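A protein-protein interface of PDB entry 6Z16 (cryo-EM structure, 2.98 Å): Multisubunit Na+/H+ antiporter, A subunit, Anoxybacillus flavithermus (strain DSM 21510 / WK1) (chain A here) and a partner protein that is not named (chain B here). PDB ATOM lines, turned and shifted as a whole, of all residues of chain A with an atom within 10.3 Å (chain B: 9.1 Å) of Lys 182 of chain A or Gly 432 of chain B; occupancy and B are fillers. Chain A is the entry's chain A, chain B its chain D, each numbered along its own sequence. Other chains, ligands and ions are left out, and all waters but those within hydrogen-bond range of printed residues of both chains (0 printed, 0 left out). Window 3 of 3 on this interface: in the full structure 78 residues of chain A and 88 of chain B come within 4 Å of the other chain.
Among the printed residues, merely in contact across the chains: Arg 187 of chain A with Met 427 of chain B (3.4 Å), Phe 181 of chain A with Trp 431 of chain B (3.6 Å), Phe 181 of chain A with Thr 364 of chain B (3.6 Å), Ala 178 of chain A with Trp 431 of chain B (3.7 Å), Arg 187 of chain A with Trp 431 of chain B (3.7 Å), Lys 182 of chain A with Gly 432 of chain B (3.95 Å) and Arg 187 of chain A with Gly 432 of chain B (3.97 Å).
The guanidinium group (NE) of Arg 187 of chain A is in hydrogen-bond range of the backbone carbonyl oxygen (O) of Phe 181 of chain A (3.3 Å). OG1 of Thr 364 of chain B lies within hydrogen-bond range of O of Gly 361 of chain B, at 3.2 Å. N of Gly 361 of chain B sits at hydrogen-bond distance from O of Trp 431 of chain B (3.3 Å).
O of Phe 181 of chain A is in hydrogen-bond range of N of Gly 432 of chain B.
Gly 432 of chain B touches just these residues of chain A: Phe 181, Lys 182 and Arg 187. Gly 361 of chain B touches none of the printed residues of chain A. Of the printed residues of chain A, Met 427 of chain B touches Arg 187 (3.4 Å). Of the printed residues of chain A, Trp 431 of chain B touches Ala 178 (3.7 Å), Phe 181 (3.6 Å) and Arg 187 (3.7 Å). Of the printed residues of chain B, Ala 178 of chain A touches Trp 431 (3.7 Å). Of the printed residues of chain B, Phe 181 of chain A touches Thr 364, Trp 431 and Gly 432. Glu 433 of chain B touches none of the printed residues of chain A. Tyr 188 of chain A touches none of the printed residues of chain B. The nearest residue of chain B that does not touch Lys 182 of chain A is Glu 433 of chain B (4.4 Å). The nearest residue of chain A that does not touch Gly 432 of chain B is Arg 183 of chain A (5.6 Å).
Hydrophobic or aromatic side chains of chain A within 4 Å of the printed part of chain B: Ala 178 and Phe 181. Hydrophobic or aromatic side chains of chain B that line the printed part of chain A: Met 427 and Trp 431. Along chain B the printed residues that touch a printed residue of chain A span positions 364 to 432. Among the printed residues, 8 pairs touch across the chains. Among the printed residues, no Asp or Glu carboxylate lies within 4 Å of a Lys or Arg side-chain nitrogen of the other chain.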
ATOM      1  N   LYS A 133      -9.427 -10.909  18.282  1.00  0.00           N
ATOM      2  CA  LYS A 133     -10.678 -10.174  18.341  1.00  0.00           C
ATOM      3  C   LYS A 133     -11.030  -9.714  19.745  1.00  0.00           C
ATOM      4  O   LYS A 133     -12.001  -8.968  19.906  1.00  0.00           O
ATOM      5  CB  LYS A 133     -11.843 -11.023  17.797  1.00  0.00           C
ATOM      6  CG  LYS A 133     -11.969 -11.096  16.271  1.00  0.00           C
ATOM      7  CD  LYS A 133     -11.013 -12.111  15.660  1.00  0.00           C
ATOM      8  CE  LYS A 133     -11.211 -12.252  14.168  1.00  0.00           C
ATOM      9  NZ  LYS A 133     -10.197 -13.167  13.577  1.00  0.00           N
ATOM     10  N   GLU A 134     -10.272 -10.129  20.756  1.00  0.00           N
ATOM     11  CA  GLU A 134     -10.581  -9.871  22.150  1.00  0.00           C
ATOM     12  C   GLU A 134      -9.381  -9.242  22.845  1.00  0.00           C
ATOM     13  O   GLU A 134      -8.241  -9.655  22.606  1.00  0.00           O
ATOM     14  CB  GLU A 134     -10.951 -11.173  22.876  1.00  0.00           C
ATOM     15  CG  GLU A 134     -12.217 -11.861  22.396  1.00  0.00           C
ATOM     16  CD  GLU A 134     -13.474 -11.129  22.796  1.00  0.00           C
ATOM     17  OE1 GLU A 134     -13.461 -10.461  23.850  1.00  0.00           O
ATOM     18  OE2 GLU A 134     -14.483 -11.241  22.071  1.00  0.00           O
ATOM     19  N   PRO A 135      -9.599  -8.246  23.695  1.00  0.00           N
ATOM     20  CA  PRO A 135      -8.540  -7.839  24.630  1.00  0.00           C
ATOM     21  C   PRO A 135      -8.381  -8.831  25.771  1.00  0.00           C
ATOM     22  O   PRO A 135      -9.207  -8.873  26.686  1.00  0.00           O
ATOM     23  CB  PRO A 135      -9.017  -6.471  25.129  1.00  0.00           C
ATOM     24  CG  PRO A 135     -10.498  -6.477  24.913  1.00  0.00           C
ATOM     25  CD  PRO A 135     -10.731  -7.304  23.684  1.00  0.00           C
ATOM     26  N   ILE A 177     -17.700  -7.738  34.973  1.00  0.00           N
ATOM     27  CA  ILE A 177     -19.058  -7.740  34.426  1.00  0.00           C
ATOM     28  C   ILE A 177     -19.161  -6.846  33.193  1.00  0.00           C
ATOM     29  O   ILE A 177     -19.847  -7.189  32.223  1.00  0.00           O
ATOM     30  CB  ILE A 177     -20.060  -7.344  35.530  1.00  0.00           C
ATOM     31  CG1 ILE A 177     -20.101  -8.426  36.598  1.00  0.00           C
ATOM     32  CG2 ILE A 177     -21.458  -7.176  34.992  1.00  0.00           C
ATOM     33  CD1 ILE A 177     -20.799  -8.013  37.851  1.00  0.00           C
ATOM     34  N   ALA A 178     -18.431  -5.735  33.168  1.00  0.00           N
ATOM     35  CA  ALA A 178     -18.485  -4.783  32.061  1.00  0.00           C
ATOM     36  C   ALA A 178     -17.356  -4.995  31.068  1.00  0.00           C
ATOM     37  O   ALA A 178     -16.773  -4.022  30.585  1.00  0.00           O
ATOM     38  CB  ALA A 178     -18.459  -3.356  32.584  1.00  0.00           C
ATOM     39  N   TYR A 179     -17.018  -6.259  30.783  1.00  0.00           N
ATOM     40  CA  TYR A 179     -15.877  -6.580  29.927  1.00  0.00           C
ATOM     41  C   TYR A 179     -16.064  -6.062  28.509  1.00  0.00           C
ATOM     42  O   TYR A 179     -15.098  -5.644  27.865  1.00  0.00           O
ATOM     43  CB  TYR A 179     -15.646  -8.091  29.919  1.00  0.00           C
ATOM     44  CG  TYR A 179     -14.508  -8.537  29.033  1.00  0.00           C
ATOM     45  CD1 TYR A 179     -13.191  -8.357  29.419  1.00  0.00           C
ATOM     46  CD2 TYR A 179     -14.757  -9.142  27.808  1.00  0.00           C
ATOM     47  CE1 TYR A 179     -12.155  -8.759  28.609  1.00  0.00           C
ATOM     48  CE2 TYR A 179     -13.728  -9.544  26.993  1.00  0.00           C
ATOM     49  CZ  TYR A 179     -12.431  -9.353  27.401  1.00  0.00           C
ATOM     50  OH  TYR A 179     -11.401  -9.757  26.593  1.00  0.00           O
ATOM     51  N   TRP A 180     -17.289  -6.080  28.005  1.00  0.00           N
ATOM     52  CA  TRP A 180     -17.611  -5.400  26.756  1.00  0.00           C
ATOM     53  C   TRP A 180     -18.201  -4.049  27.131  1.00  0.00           C
ATOM     54  O   TRP A 180     -19.394  -3.927  27.391  1.00  0.00           O
ATOM     55  CB  TRP A 180     -18.579  -6.206  25.904  1.00  0.00           C
ATOM     56  CG  TRP A 180     -18.025  -7.468  25.344  1.00  0.00           C
ATOM     57  CD1 TRP A 180     -17.231  -7.595  24.246  1.00  0.00           C
ATOM     58  CD2 TRP A 180     -18.287  -8.795  25.803  1.00  0.00           C
ATOM     59  NE1 TRP A 180     -16.945  -8.915  24.017  1.00  0.00           N
ATOM     60  CE2 TRP A 180     -17.587  -9.674  24.958  1.00  0.00           C
ATOM     61  CE3 TRP A 180     -19.033  -9.325  26.857  1.00  0.00           C
ATOM     62  CZ2 TRP A 180     -17.611 -11.051  25.133  1.00  0.00           C
ATOM     63  CZ3 TRP A 180     -19.056 -10.692  27.029  1.00  0.00           C
ATOM     64  CH2 TRP A 180     -18.349 -11.540  26.173  1.00  0.00           C
ATOM     65  N   PHE A 181     -17.357  -3.022  27.161  1.00  0.00           N
ATOM     66  CA  PHE A 181     -17.815  -1.707  27.579  1.00  0.00           C
ATOM     67  C   PHE A 181     -18.537  -0.949  26.474  1.00  0.00           C
ATOM     68  O   PHE A 181     -19.199   0.047  26.769  1.00  0.00           O
ATOM     69  CB  PHE A 181     -16.643  -0.881  28.128  1.00  0.00           C
ATOM     70  CG  PHE A 181     -15.500  -0.698  27.161  1.00  0.00           C
ATOM     71  CD1 PHE A 181     -14.445  -1.594  27.140  1.00  0.00           C
ATOM     72  CD2 PHE A 181     -15.463   0.386  26.299  1.00  0.00           C
ATOM     73  CE1 PHE A 181     -13.399  -1.429  26.262  1.00  0.00           C
ATOM     74  CE2 PHE A 181     -14.421   0.552  25.420  1.00  0.00           C
ATOM     75  CZ  PHE A 181     -13.388  -0.355  25.402  1.00  0.00           C
ATOM     76  N   LYS A 182     -18.458  -1.401  25.229  1.00  0.00           N
ATOM     77  CA  LYS A 182     -19.141  -0.730  24.131  1.00  0.00           C
ATOM     78  C   LYS A 182     -20.610  -1.113  24.004  1.00  0.00           C
ATOM     79  O   LYS A 182     -21.238  -0.748  23.005  1.00  0.00           O
ATOM     80  CB  LYS A 182     -18.437  -1.013  22.800  1.00  0.00           C
ATOM     81  CG  LYS A 182     -17.052  -0.411  22.675  1.00  0.00           C
ATOM     82  CD  LYS A 182     -16.560  -0.433  21.235  1.00  0.00           C
ATOM     83  CE  LYS A 182     -16.172  -1.821  20.791  1.00  0.00           C
ATOM     84  NZ  LYS A 182     -15.572  -1.825  19.429  1.00  0.00           N
ATOM     85  N   ARG A 183     -21.176  -1.840  24.964  1.00  0.00           N
ATOM     86  CA  ARG A 183     -22.585  -2.202  24.931  1.00  0.00           C
ATOM     87  C   ARG A 183     -23.252  -1.733  26.217  1.00  0.00           C
ATOM     88  O   ARG A 183     -22.633  -1.733  27.284  1.00  0.00           O
ATOM     89  CB  ARG A 183     -22.772  -3.714  24.709  1.00  0.00           C
ATOM     90  CG  ARG A 183     -22.203  -4.599  25.791  1.00  0.00           C
ATOM     91  CD  ARG A 183     -22.334  -6.080  25.460  1.00  0.00           C
ATOM     92  NE  ARG A 183     -21.518  -6.472  24.312  1.00  0.00           N
ATOM     93  CZ  ARG A 183     -21.469  -7.704  23.815  1.00  0.00           C
ATOM     94  NH1 ARG A 183     -20.702  -7.969  22.767  1.00  0.00           N
ATOM     95  NH2 ARG A 183     -22.170  -8.678  24.376  1.00  0.00           N
ATOM     96  N   ASP A 184     -24.517  -1.315  26.098  1.00  0.00           N
ATOM     97  CA  ASP A 184     -25.159  -0.541  27.157  1.00  0.00           C
ATOM     98  C   ASP A 184     -25.528  -1.407  28.351  1.00  0.00           C
ATOM     99  O   ASP A 184     -25.309  -1.011  29.504  1.00  0.00           O
ATOM    100  CB  ASP A 184     -26.409   0.149  26.614  1.00  0.00           C
ATOM    101  CG  ASP A 184     -26.092   1.215  25.584  1.00  0.00           C
ATOM    102  OD1 ASP A 184     -25.002   1.816  25.655  1.00  0.00           O
ATOM    103  OD2 ASP A 184     -26.941   1.456  24.701  1.00  0.00           O
ATOM    104  N   ARG A 185     -26.085  -2.591  28.087  1.00  0.00           N
ATOM    105  CA  ARG A 185     -26.631  -3.435  29.141  1.00  0.00           C
ATOM    106  C   ARG A 185     -25.550  -3.973  30.072  1.00  0.00           C
ATOM    107  O   ARG A 185     -25.811  -4.180  31.264  1.00  0.00           O
ATOM    108  CB  ARG A 185     -27.442  -4.557  28.500  1.00  0.00           C
ATOM    109  CG  ARG A 185     -26.647  -5.423  27.554  1.00  0.00           C
ATOM    110  CD  ARG A 185     -27.536  -6.349  26.749  1.00  0.00           C
ATOM    111  NE  ARG A 185     -26.740  -7.289  25.967  1.00  0.00           N
ATOM    112  CZ  ARG A 185     -26.251  -7.031  24.759  1.00  0.00           C
ATOM    113  NH1 ARG A 185     -26.477  -5.858  24.183  1.00  0.00           N
ATOM    114  NH2 ARG A 185     -25.534  -7.948  24.125  1.00  0.00           N
ATOM    115  N   SER A 186     -24.324  -4.140  29.568  1.00  0.00           N
ATOM    116  CA  SER A 186     -23.205  -4.498  30.431  1.00  0.00           C
ATOM    117  C   SER A 186     -22.869  -3.369  31.391  1.00  0.00           C
ATOM    118  O   SER A 186     -22.550  -3.616  32.559  1.00  0.00           O
ATOM    119  CB  SER A 186     -21.987  -4.850  29.587  1.00  0.00           C
ATOM    120  OG  SER A 186     -22.237  -5.999  28.804  1.00  0.00           O
ATOM    121  N   ARG A 187     -22.980  -2.122  30.930  1.00  0.00           N
ATOM    122  CA  ARG A 187     -22.693  -0.990  31.802  1.00  0.00           C
ATOM    123  C   ARG A 187     -23.791  -0.790  32.838  1.00  0.00           C
ATOM    124  O   ARG A 187     -23.496  -0.456  33.991  1.00  0.00           O
ATOM    125  CB  ARG A 187     -22.477   0.270  30.969  1.00  0.00           C
ATOM    126  CG  ARG A 187     -21.167   0.239  30.225  1.00  0.00           C
ATOM    127  CD  ARG A 187     -20.871   1.520  29.485  1.00  0.00           C
ATOM    128  NE  ARG A 187     -21.653   1.670  28.266  1.00  0.00           N
ATOM    129  CZ  ARG A 187     -22.536   2.636  28.066  1.00  0.00           C
ATOM    130  NH1 ARG A 187     -23.195   2.703  26.923  1.00  0.00           N
ATOM    131  NH2 ARG A 187     -22.749   3.542  29.007  1.00  0.00           N
ATOM    132  N   TYR A 188     -25.056  -1.018  32.451  1.00  0.00           N
ATOM    133  CA  TYR A 188     -26.153  -0.982  33.420  1.00  0.00           C
ATOM    134  C   TYR A 188     -25.977  -2.048  34.494  1.00  0.00           C
ATOM    135  O   TYR A 188     -26.133  -1.770  35.692  1.00  0.00           O
ATOM    136  CB  TYR A 188     -27.511  -1.171  32.737  1.00  0.00           C
ATOM    137  CG  TYR A 188     -27.978  -0.041  31.851  1.00  0.00           C
ATOM    138  CD1 TYR A 188     -28.327   1.193  32.389  1.00  0.00           C
ATOM    139  CD2 TYR A 188     -28.173  -0.237  30.493  1.00  0.00           C
ATOM    140  CE1 TYR A 188     -28.781   2.221  31.582  1.00  0.00           C
ATOM    141  CE2 TYR A 188     -28.628   0.782  29.677  1.00  0.00           C
ATOM    142  CZ  TYR A 188     -28.932   2.006  30.227  1.00  0.00           C
ATOM    143  OH  TYR A 188     -29.390   3.019  29.417  1.00  0.00           O
ATOM    144  N   GLU A 263     -24.584 -10.444  31.703  1.00  0.00           N
ATOM    145  CA  GLU A 263     -24.036  -9.948  30.450  1.00  0.00           C
ATOM    146  C   GLU A 263     -22.520 -10.018  30.421  1.00  0.00           C
ATOM    147  O   GLU A 263     -21.901  -9.519  29.479  1.00  0.00           O
ATOM    148  CB  GLU A 263     -24.507  -8.518  30.192  1.00  0.00           C
ATOM    149  CG  GLU A 263     -25.996  -8.423  29.949  1.00  0.00           C
ATOM    150  CD  GLU A 263     -26.424  -9.122  28.676  1.00  0.00           C
ATOM    151  OE1 GLU A 263     -25.659  -9.091  27.691  1.00  0.00           O
ATOM    152  OE2 GLU A 263     -27.521  -9.718  28.665  1.00  0.00           O
ATOM    153  N   PHE B 359     -20.170  13.025  25.323  1.00  0.00           N
ATOM    154  CA  PHE B 359     -19.031  12.277  24.819  1.00  0.00           C
ATOM    155  C   PHE B 359     -18.939  10.932  25.515  1.00  0.00           C
ATOM    156  O   PHE B 359     -19.354  10.782  26.666  1.00  0.00           O
ATOM    157  CB  PHE B 359     -17.724  13.065  25.009  1.00  0.00           C
ATOM    158  CG  PHE B 359     -17.361  13.335  26.448  1.00  0.00           C
ATOM    159  CD1 PHE B 359     -17.854  14.444  27.102  1.00  0.00           C
ATOM    160  CD2 PHE B 359     -16.476  12.515  27.123  1.00  0.00           C
ATOM    161  CE1 PHE B 359     -17.512  14.701  28.409  1.00  0.00           C
ATOM    162  CE2 PHE B 359     -16.137  12.769  28.431  1.00  0.00           C
ATOM    163  CZ  PHE B 359     -16.651  13.866  29.071  1.00  0.00           C
ATOM    164  N   SER B 360     -18.365   9.960  24.810  1.00  0.00           N
ATOM    165  CA  SER B 360     -18.126   8.637  25.367  1.00  0.00           C
ATOM    166  C   SER B 360     -17.012   7.963  24.583  1.00  0.00           C
ATOM    167  O   SER B 360     -16.774   8.285  23.418  1.00  0.00           O
ATOM    168  CB  SER B 360     -19.395   7.779  25.338  1.00  0.00           C
ATOM    169  OG  SER B 360     -19.818   7.546  24.007  1.00  0.00           O
ATOM    170  N   GLY B 361     -16.334   7.028  25.237  1.00  0.00           N
ATOM    171  CA  GLY B 361     -15.355   6.203  24.561  1.00  0.00           C
ATOM    172  C   GLY B 361     -13.935   6.725  24.604  1.00  0.00           C
ATOM    173  O   GLY B 361     -13.277   6.807  23.566  1.00  0.00           O
ATOM    174  N   LEU B 362     -13.440   7.057  25.794  1.00  0.00           N
ATOM    175  CA  LEU B 362     -12.101   7.608  25.930  1.00  0.00           C
ATOM    176  C   LEU B 362     -11.048   6.571  26.297  1.00  0.00           C
ATOM    177  O   LEU B 362      -9.857   6.849  26.135  1.00  0.00           O
ATOM    178  CB  LEU B 362     -12.082   8.715  26.988  1.00  0.00           C
ATOM    179  CG  LEU B 362     -12.822  10.045  26.835  1.00  0.00           C
ATOM    180  CD1 LEU B 362     -12.745  10.790  28.145  1.00  0.00           C
ATOM    181  CD2 LEU B 362     -12.235  10.890  25.745  1.00  0.00           C
ATOM    182  N   ILE B 363     -11.454   5.401  26.798  1.00  0.00           N
ATOM    183  CA  ILE B 363     -10.520   4.309  27.071  1.00  0.00           C
ATOM    184  C   ILE B 363      -9.890   3.791  25.785  1.00  0.00           C
ATOM    185  O   ILE B 363      -8.697   3.466  25.755  1.00  0.00           O
ATOM    186  CB  ILE B 363     -11.242   3.199  27.867  1.00  0.00           C
ATOM    187  CG1 ILE B 363     -11.471   3.643  29.302  1.00  0.00           C
ATOM    188  CG2 ILE B 363     -10.485   1.884  27.871  1.00  0.00           C
ATOM    189  CD1 ILE B 363     -10.198   3.861  30.054  1.00  0.00           C
ATOM    190  N   THR B 364     -10.645   3.781  24.686  1.00  0.00           N
ATOM    191  CA  THR B 364     -10.112   3.303  23.415  1.00  0.00           C
ATOM    192  C   THR B 364      -9.061   4.227  22.814  1.00  0.00           C
ATOM    193  O   THR B 364      -8.396   3.828  21.854  1.00  0.00           O
ATOM    194  CB  THR B 364     -11.237   3.121  22.399  1.00  0.00           C
ATOM    195  OG1 THR B 364     -11.792   4.398  22.065  1.00  0.00           O
ATOM    196  CG2 THR B 364     -12.328   2.265  22.983  1.00  0.00           C
ATOM    197  N   SER B 365      -8.895   5.438  23.341  1.00  0.00           N
ATOM    198  CA  SER B 365      -7.914   6.381  22.833  1.00  0.00           C
ATOM    199  C   SER B 365      -6.999   6.961  23.895  1.00  0.00           C
ATOM    200  O   SER B 365      -5.919   7.443  23.541  1.00  0.00           O
ATOM    201  CB  SER B 365      -8.612   7.535  22.107  1.00  0.00           C
ATOM    202  OG  SER B 365      -9.309   7.060  20.973  1.00  0.00           O
ATOM    203  N   PHE B 426     -16.706   8.452  35.275  1.00  0.00           N
ATOM    204  CA  PHE B 426     -15.878   7.422  34.639  1.00  0.00           C
ATOM    205  C   PHE B 426     -16.679   6.525  33.700  1.00  0.00           C
ATOM    206  O   PHE B 426     -16.233   6.231  32.588  1.00  0.00           O
ATOM    207  CB  PHE B 426     -15.178   6.571  35.697  1.00  0.00           C
ATOM    208  CG  PHE B 426     -14.383   5.433  35.122  1.00  0.00           C
ATOM    209  CD1 PHE B 426     -13.188   5.668  34.473  1.00  0.00           C
ATOM    210  CD2 PHE B 426     -14.828   4.126  35.234  1.00  0.00           C
ATOM    211  CE1 PHE B 426     -12.458   4.629  33.934  1.00  0.00           C
ATOM    212  CE2 PHE B 426     -14.102   3.083  34.699  1.00  0.00           C
ATOM    213  CZ  PHE B 426     -12.914   3.337  34.052  1.00  0.00           C
ATOM    214  N   MET B 427     -17.856   6.078  34.122  1.00  0.00           N
ATOM    215  CA  MET B 427     -18.613   5.123  33.333  1.00  0.00           C
ATOM    216  C   MET B 427     -19.315   5.763  32.153  1.00  0.00           C
ATOM    217  O   MET B 427     -19.469   5.114  31.116  1.00  0.00           O
ATOM    218  CB  MET B 427     -19.637   4.405  34.202  1.00  0.00           C
ATOM    219  CG  MET B 427     -19.029   3.475  35.209  1.00  0.00           C
ATOM    220  SD  MET B 427     -20.298   2.665  36.173  1.00  0.00           S
ATOM    221  CE  MET B 427     -20.962   1.584  34.918  1.00  0.00           C
ATOM    222  N   ASN B 428     -19.762   7.012  32.267  1.00  0.00           N
ATOM    223  CA  ASN B 428     -20.394   7.613  31.106  1.00  0.00           C
ATOM    224  C   ASN B 428     -19.395   8.280  30.176  1.00  0.00           C
ATOM    225  O   ASN B 428     -19.650   8.368  28.972  1.00  0.00           O
ATOM    226  CB  ASN B 428     -21.450   8.622  31.546  1.00  0.00           C
ATOM    227  CG  ASN B 428     -22.577   7.985  32.316  1.00  0.00           C
ATOM    228  OD1 ASN B 428     -22.760   8.247  33.502  1.00  0.00           O
ATOM    229  ND2 ASN B 428     -23.349   7.145  31.645  1.00  0.00           N
ATOM    230  N   GLY B 429     -18.260   8.738  30.698  1.00  0.00           N
ATOM    231  CA  GLY B 429     -17.280   9.401  29.867  1.00  0.00           C
ATOM    232  C   GLY B 429     -16.302   8.465  29.194  1.00  0.00           C
ATOM    233  O   GLY B 429     -16.108   8.537  27.982  1.00  0.00           O
ATOM    234  N   PHE B 430     -15.686   7.572  29.966  1.00  0.00           N
ATOM    235  CA  PHE B 430     -14.613   6.752  29.425  1.00  0.00           C
ATOM    236  C   PHE B 430     -15.137   5.508  28.713  1.00  0.00           C
ATOM    237  O   PHE B 430     -14.670   5.181  27.618  1.00  0.00           O
ATOM    238  CB  PHE B 430     -13.638   6.387  30.543  1.00  0.00           C
ATOM    239  CG  PHE B 430     -12.829   7.554  31.043  1.00  0.00           C
ATOM    240  CD1 PHE B 430     -11.690   7.957  30.375  1.00  0.00           C
ATOM    241  CD2 PHE B 430     -13.214   8.254  32.170  1.00  0.00           C
ATOM    242  CE1 PHE B 430     -10.955   9.035  30.816  1.00  0.00           C
ATOM    243  CE2 PHE B 430     -12.476   9.324  32.623  1.00  0.00           C
ATOM    244  CZ  PHE B 430     -11.346   9.713  31.947  1.00  0.00           C
ATOM    245  N   TRP B 431     -16.108   4.810  29.291  1.00  0.00           N
ATOM    246  CA  TRP B 431     -16.687   3.653  28.626  1.00  0.00           C
ATOM    247  C   TRP B 431     -17.691   4.081  27.559  1.00  0.00           C
ATOM    248  O   TRP B 431     -18.010   5.259  27.402  1.00  0.00           O
ATOM    249  CB  TRP B 431     -17.348   2.728  29.643  1.00  0.00           C
ATOM    250  CG  TRP B 431     -16.381   1.910  30.431  1.00  0.00           C
ATOM    251  CD1 TRP B 431     -15.058   1.744  30.176  1.00  0.00           C
ATOM    252  CD2 TRP B 431     -16.662   1.149  31.607  1.00  0.00           C
ATOM    253  NE1 TRP B 431     -14.493   0.921  31.114  1.00  0.00           N
ATOM    254  CE2 TRP B 431     -15.458   0.546  32.008  1.00  0.00           C
ATOM    255  CE3 TRP B 431     -17.813   0.921  32.361  1.00  0.00           C
ATOM    256  CZ2 TRP B 431     -15.373  -0.276  33.126  1.00  0.00           C
ATOM    257  CZ3 TRP B 431     -17.726   0.108  33.472  1.00  0.00           C
ATOM    258  CH2 TRP B 431     -16.515  -0.481  33.845  1.00  0.00           C
ATOM    259  N   GLY B 432     -18.194   3.103  26.817  1.00  0.00           N
ATOM    260  CA  GLY B 432     -19.116   3.354  25.725  1.00  0.00           C
ATOM    261  C   GLY B 432     -18.410   3.391  24.387  1.00  0.00           C
ATOM    262  O   GLY B 432     -17.198   3.198  24.275  1.00  0.00           O
ATOM    263  N   GLU B 433     -19.193   3.645  23.344  1.00  0.00           N
ATOM    264  CA  GLU B 433     -18.614   3.793  22.019  1.00  0.00           C
ATOM    265  C   GLU B 433     -18.177   5.238  21.791  1.00  0.00           C
ATOM    266  O   GLU B 433     -18.535   6.149  22.533  1.00  0.00           O
ATOM    267  CB  GLU B 433     -19.600   3.369  20.933  1.00  0.00           C
ATOM    268  CG  GLU B 433     -20.767   4.319  20.754  1.00  0.00           C
ATOM    269  CD  GLU B 433     -21.673   3.923  19.607  1.00  0.00           C
ATOM    270  OE1 GLU B 433     -21.395   2.896  18.954  1.00  0.00           O
ATOM    271  OE2 GLU B 433     -22.660   4.642  19.356  1.00  0.00           O
ATOM    272  N   LYS B 434     -17.412   5.444  20.726  1.00  0.00           N
ATOM    273  CA  LYS B 434     -16.797   6.733  20.424  1.00  0.00           C
ATOM    274  C   LYS B 434     -17.779   7.615  19.664  1.00  0.00           C
ATOM    275  O   LYS B 434     -18.140   7.306  18.525  1.00  0.00           O
ATOM    276  CB  LYS B 434     -15.532   6.520  19.600  1.00  0.00           C
ATOM    277  CG  LYS B 434     -14.854   7.796  19.154  1.00  0.00           C
ATOM    278  CD  LYS B 434     -13.589   7.500  18.382  1.00  0.00           C
ATOM    279  CE  LYS B 434     -12.993   8.772  17.822  1.00  0.00           C
ATOM    280  NZ  LYS B 434     -12.523   9.664  18.904  1.00  0.00           N
ATOM    281  N   LYS B 435     -18.209   8.720  20.281  1.00  0.00           N
ATOM    282  CA  LYS B 435     -19.006   9.694  19.534  1.00  0.00           C
ATOM    283  C   LYS B 435     -18.629  11.151  19.758  1.00  0.00           C
ATOM    284  O   LYS B 435     -18.912  11.970  18.878  1.00  0.00           O
ATOM    285  CB  LYS B 435     -20.501   9.533  19.847  1.00  0.00           C
ATOM    286  CG  LYS B 435     -20.906   9.961  21.245  1.00  0.00           C
ATOM    287  CD  LYS B 435     -22.393   9.817  21.470  1.00  0.00           C
ATOM    288  CE  LYS B 435     -22.785  10.353  22.835  1.00  0.00           C
ATOM    289  NZ  LYS B 435     -22.196   9.545  23.932  1.00  0.00           N
ATOM    290  N   GLY B 436     -18.000  11.525  20.866  1.00  0.00           N
ATOM    291  CA  GLY B 436     -18.037  12.920  21.255  1.00  0.00           C
ATOM    292  C   GLY B 436     -16.868  13.795  20.863  1.00  0.00           C
ATOM    293  O   GLY B 436     -17.019  15.012  20.733  1.00  0.00           O
ATOM    294  N   PHE B 437     -15.703  13.196  20.663  1.00  0.00           N
ATOM    295  CA  PHE B 437     -14.451  13.930  20.611  1.00  0.00           C
ATOM    296  C   PHE B 437     -13.704  13.573  19.335  1.00  0.00           C
ATOM    297  O   PHE B 437     -14.118  12.705  18.565  1.00  0.00           O
ATOM    298  CB  PHE B 437     -13.614  13.644  21.866  1.00  0.00           C
ATOM    299  CG  PHE B 437     -13.128  12.220  21.980  1.00  0.00           C
ATOM    300  CD1 PHE B 437     -13.956  11.215  22.459  1.00  0.00           C
ATOM    301  CD2 PHE B 437     -11.816  11.902  21.682  1.00  0.00           C
ATOM    302  CE1 PHE B 437     -13.508   9.919  22.567  1.00  0.00           C
ATOM    303  CE2 PHE B 437     -11.358  10.609  21.807  1.00  0.00           C
ATOM    304  CZ  PHE B 437     -12.206   9.619  22.252  1.00  0.00           C
